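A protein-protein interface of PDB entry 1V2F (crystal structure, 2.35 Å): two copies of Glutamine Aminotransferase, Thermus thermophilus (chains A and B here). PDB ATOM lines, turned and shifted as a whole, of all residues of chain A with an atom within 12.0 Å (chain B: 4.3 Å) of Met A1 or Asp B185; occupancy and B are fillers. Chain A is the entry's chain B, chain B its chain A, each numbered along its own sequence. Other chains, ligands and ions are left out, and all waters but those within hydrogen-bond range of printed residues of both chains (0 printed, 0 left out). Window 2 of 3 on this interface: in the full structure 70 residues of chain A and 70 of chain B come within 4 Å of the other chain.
Met A1 touches Leu B186 (CE to O, 3.6 Å). Phe B187 touches Met A1. Met A1 touches Arg B213. Phe B187 touches Arg A2 (CE2 to O, 3.5 Å).
Met A1 touches four residues of chain B. Leu B186 touches just one residue of chain A: Met A1 (3.6 Å). Arg B213 touches just one residue of chain A: Met A1 (2.8 Å). Of the printed residues of chain B, Arg A2 touches Phe B187 (3.5 Å). Pro A5 touches none of the printed residues of chain B. Thr A7 touches none of the printed residues of chain B. The nearest printed residue of chain B that does not touch Met A1 is Ala B181 (6.0 Å). The nearest printed residue of chain B that does not touch Arg A2 is Asp B185 (5.7 Å).
Hydrophobic or aromatic side chains of chain A that line the printed part of chain B: Met A1. Of the 8 printed residues of chain B, 4 touch a printed residue of chain A. Hydrophobic or aromatic side chains of chain B within 4 Å of the printed part of chain A: Phe B187. Among the printed residues, no Asp or Glu carboxylate lies within 4 Å of a Lys or Arg side-chain nitrogen of the other chain.
The side-chain carboxylate (OD2) of Asp B185 sits at hydrogen-bond distance from the backbone NH (N) of Met A1, at 2.8 Å.
No position is printed for both chains. Of the 5 pairs that touch across the chains among the printed residues, none has its exchanged pair printed and touching as well.
O of Leu B186 is in hydrogen-bond range of NH1 of Arg B213, at 3.1 Å. The backbone carbonyl oxygen (O) of Ala B181 lies within hydrogen-bond range of the backbone NH (N) of Leu B186, at 2.7 Å. The side-chain carboxylate (OD1) of Asp B185 lies within salt-bridge range of the guanidinium group (NH1) of Arg B213, at 3.3 Å.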
ATOM      1  N   MET A   1      27.825   7.005 -19.592  1.00  0.00           N
ATOM      2  CA  MET A   1      27.436   6.756 -21.014  1.00  0.00           C
ATOM      3  C   MET A   1      27.013   5.311 -21.242  1.00  0.00           C
ATOM      4  O   MET A   1      27.708   4.377 -20.843  1.00  0.00           O
ATOM      5  CB  MET A   1      28.604   7.073 -21.951  1.00  0.00           C
ATOM      6  CG  MET A   1      29.864   6.279 -21.640  1.00  0.00           C
ATOM      7  SD  MET A   1      31.067   6.287 -22.981  1.00  0.00           S
ATOM      8  CE  MET A   1      31.056   8.009 -23.405  1.00  0.00           C
ATOM      9  N   ARG A   2      25.869   5.134 -21.889  1.00  0.00           N
ATOM     10  CA  ARG A   2      25.372   3.802 -22.189  1.00  0.00           C
ATOM     11  C   ARG A   2      24.595   3.846 -23.499  1.00  0.00           C
ATOM     12  O   ARG A   2      24.199   4.919 -23.964  1.00  0.00           O
ATOM     13  CB  ARG A   2      24.468   3.283 -21.063  1.00  0.00           C
ATOM     14  CG  ARG A   2      23.029   3.805 -21.088  1.00  0.00           C
ATOM     15  CD  ARG A   2      22.948   5.299 -20.804  1.00  0.00           C
ATOM     16  NE  ARG A   2      21.567   5.748 -20.606  1.00  0.00           N
ATOM     17  CZ  ARG A   2      20.652   5.835 -21.570  1.00  0.00           C
ATOM     18  NH1 ARG A   2      20.961   5.510 -22.821  1.00  0.00           N
ATOM     19  NH2 ARG A   2      19.420   6.243 -21.281  1.00  0.00           N
ATOM     20  N   LEU A   3      24.383   2.676 -24.089  1.00  0.00           N
ATOM     21  CA  LEU A   3      23.656   2.589 -25.342  1.00  0.00           C
ATOM     22  C   LEU A   3      22.175   2.814 -25.095  1.00  0.00           C
ATOM     23  O   LEU A   3      21.672   2.540 -24.004  1.00  0.00           O
ATOM     24  CB  LEU A   3      23.870   1.216 -25.989  1.00  0.00           C
ATOM     25  CG  LEU A   3      25.309   0.866 -26.378  1.00  0.00           C
ATOM     26  CD1 LEU A   3      25.332  -0.491 -27.060  1.00  0.00           C
ATOM     27  CD2 LEU A   3      25.870   1.942 -27.303  1.00  0.00           C
ATOM     28  N   HIS A   4      21.481   3.316 -26.110  1.00  0.00           N
ATOM     29  CA  HIS A   4      20.052   3.567 -26.006  1.00  0.00           C
ATOM     30  C   HIS A   4      19.309   2.261 -25.727  1.00  0.00           C
ATOM     31  O   HIS A   4      19.665   1.212 -26.260  1.00  0.00           O
ATOM     32  CB  HIS A   4      19.543   4.201 -27.296  1.00  0.00           C
ATOM     33  CG  HIS A   4      18.117   4.637 -27.225  1.00  0.00           C
ATOM     34  ND1 HIS A   4      17.065   3.748 -27.270  1.00  0.00           N
ATOM     35  CD2 HIS A   4      17.567   5.868 -27.102  1.00  0.00           C
ATOM     36  CE1 HIS A   4      15.927   4.415 -27.181  1.00  0.00           C
ATOM     37  NE2 HIS A   4      16.204   5.702 -27.079  1.00  0.00           N
ATOM     38  N   PRO A   5      18.263   2.313 -24.883  1.00  0.00           N
ATOM     39  CA  PRO A   5      17.444   1.153 -24.502  1.00  0.00           C
ATOM     40  C   PRO A   5      16.935   0.308 -25.666  1.00  0.00           C
ATOM     41  O   PRO A   5      16.670  -0.880 -25.510  1.00  0.00           O
ATOM     42  CB  PRO A   5      16.305   1.788 -23.709  1.00  0.00           C
ATOM     43  CG  PRO A   5      16.981   2.931 -23.039  1.00  0.00           C
ATOM     44  CD  PRO A   5      17.812   3.518 -24.163  1.00  0.00           C
ATOM     45  N   THR A   7      18.471  -0.887 -27.965  1.00  0.00           N
ATOM     46  CA  THR A   7      19.418  -1.970 -28.211  1.00  0.00           C
ATOM     47  C   THR A   7      19.104  -3.263 -27.459  1.00  0.00           C
ATOM     48  O   THR A   7      19.898  -4.201 -27.496  1.00  0.00           O
ATOM     49  CB  THR A   7      20.873  -1.550 -27.872  1.00  0.00           C
ATOM     50  OG1 THR A   7      20.958  -1.174 -26.493  1.00  0.00           O
ATOM     51  CG2 THR A   7      21.315  -0.374 -28.747  1.00  0.00           C
ATOM     52  N   ALA B 181      34.175  16.159 -25.304  1.00  0.00           N
ATOM     53  CA  ALA B 181      33.480  14.881 -25.280  1.00  0.00           C
ATOM     54  C   ALA B 181      33.565  14.262 -23.890  1.00  0.00           C
ATOM     55  O   ALA B 181      32.574  13.784 -23.352  1.00  0.00           O
ATOM     56  CB  ALA B 181      34.085  13.940 -26.314  1.00  0.00           C
ATOM     57  N   ARG B 182      34.758  14.277 -23.311  1.00  0.00           N
ATOM     58  CA  ARG B 182      34.959  13.708 -21.988  1.00  0.00           C
ATOM     59  C   ARG B 182      34.261  14.518 -20.898  1.00  0.00           C
ATOM     60  O   ARG B 182      33.561  13.961 -20.051  1.00  0.00           O
ATOM     61  CB  ARG B 182      36.459  13.593 -21.700  1.00  0.00           C
ATOM     62  CG  ARG B 182      37.097  12.402 -22.398  1.00  0.00           C
ATOM     63  CD  ARG B 182      38.617  12.455 -22.388  1.00  0.00           C
ATOM     64  NE  ARG B 182      39.184  11.146 -22.695  1.00  0.00           N
ATOM     65  CZ  ARG B 182      40.483  10.898 -22.835  1.00  0.00           C
ATOM     66  NH1 ARG B 182      40.899   9.666 -23.108  1.00  0.00           N
ATOM     67  NH2 ARG B 182      41.367  11.879 -22.713  1.00  0.00           N
ATOM     68  N   ALA B 183      34.437  15.833 -20.936  1.00  0.00           N
ATOM     69  CA  ALA B 183      33.824  16.717 -19.948  1.00  0.00           C
ATOM     70  C   ALA B 183      32.314  16.519 -19.832  1.00  0.00           C
ATOM     71  O   ALA B 183      31.766  16.583 -18.731  1.00  0.00           O
ATOM     72  CB  ALA B 183      34.138  18.173 -20.284  1.00  0.00           C
ATOM     73  N   HIS B 184      31.638  16.284 -20.956  1.00  0.00           N
ATOM     74  CA  HIS B 184      30.188  16.082 -20.935  1.00  0.00           C
ATOM     75  C   HIS B 184      29.782  14.619 -21.125  1.00  0.00           C
ATOM     76  O   HIS B 184      28.601  14.311 -21.272  1.00  0.00           O
ATOM     77  CB  HIS B 184      29.508  16.941 -22.001  1.00  0.00           C
ATOM     78  CG  HIS B 184      29.728  18.413 -21.827  1.00  0.00           C
ATOM     79  ND1 HIS B 184      30.961  19.009 -21.997  1.00  0.00           N
ATOM     80  CD2 HIS B 184      28.869  19.411 -21.511  1.00  0.00           C
ATOM     81  CE1 HIS B 184      30.851  20.310 -21.794  1.00  0.00           C
ATOM     82  NE2 HIS B 184      29.592  20.581 -21.498  1.00  0.00           N
ATOM     83  N   ASP B 185      30.763  13.723 -21.112  1.00  0.00           N
ATOM     84  CA  ASP B 185      30.506  12.293 -21.280  1.00  0.00           C
ATOM     85  C   ASP B 185      29.702  11.994 -22.552  1.00  0.00           C
ATOM     86  O   ASP B 185      28.690  11.291 -22.511  1.00  0.00           O
ATOM     87  CB  ASP B 185      29.766  11.749 -20.052  1.00  0.00           C
ATOM     88  CG  ASP B 185      29.717  10.234 -20.022  1.00  0.00           C
ATOM     89  OD1 ASP B 185      30.765   9.597 -20.265  1.00  0.00           O
ATOM     90  OD2 ASP B 185      28.635   9.677 -19.743  1.00  0.00           O
ATOM     91  N   LEU B 186      30.168  12.525 -23.680  1.00  0.00           N
ATOM     92  CA  LEU B 186      29.497  12.330 -24.967  1.00  0.00           C
ATOM     93  C   LEU B 186      30.078  11.180 -25.788  1.00  0.00           C
ATOM     94  O   LEU B 186      31.237  10.802 -25.615  1.00  0.00           O
ATOM     95  CB  LEU B 186      29.610  13.600 -25.812  1.00  0.00           C
ATOM     96  CG  LEU B 186      29.051  14.908 -25.264  1.00  0.00           C
ATOM     97  CD1 LEU B 186      29.361  16.041 -26.241  1.00  0.00           C
ATOM     98  CD2 LEU B 186      27.556  14.767 -25.053  1.00  0.00           C
ATOM     99  N   PHE B 187      29.264  10.632 -26.687  1.00  0.00           N
ATOM    100  CA  PHE B 187      29.719   9.572 -27.587  1.00  0.00           C
ATOM    101  C   PHE B 187      30.240  10.295 -28.816  1.00  0.00           C
ATOM    102  O   PHE B 187      29.655  11.289 -29.249  1.00  0.00           O
ATOM    103  CB  PHE B 187      28.571   8.662 -28.017  1.00  0.00           C
ATOM    104  CG  PHE B 187      28.381   7.461 -27.141  1.00  0.00           C
ATOM    105  CD1 PHE B 187      29.407   6.542 -26.969  1.00  0.00           C
ATOM    106  CD2 PHE B 187      27.156   7.222 -26.520  1.00  0.00           C
ATOM    107  CE1 PHE B 187      29.218   5.391 -26.193  1.00  0.00           C
ATOM    108  CE2 PHE B 187      26.957   6.076 -25.742  1.00  0.00           C
ATOM    109  CZ  PHE B 187      27.993   5.159 -25.581  1.00  0.00           C
ATOM    110  N   ARG B 213      35.471   6.389 -26.115  1.00  0.00           N
ATOM    111  CA  ARG B 213      34.152   6.848 -26.538  1.00  0.00           C
ATOM    112  C   ARG B 213      34.018   7.165 -28.036  1.00  0.00           C
ATOM    113  O   ARG B 213      33.036   7.786 -28.457  1.00  0.00           O
ATOM    114  CB  ARG B 213      33.793   8.094 -25.725  1.00  0.00           C
ATOM    115  CG  ARG B 213      34.796   9.236 -25.926  1.00  0.00           C
ATOM    116  CD  ARG B 213      34.660  10.341 -24.881  1.00  0.00           C
ATOM    117  NE  ARG B 213      34.846   9.820 -23.530  1.00  0.00           N
ATOM    118  CZ  ARG B 213      33.884   9.767 -22.617  1.00  0.00           C
ATOM    119  NH1 ARG B 213      32.668  10.209 -22.908  1.00  0.00           N
ATOM    120  NH2 ARG B 213      34.136   9.264 -21.419  1.00  0.00           N
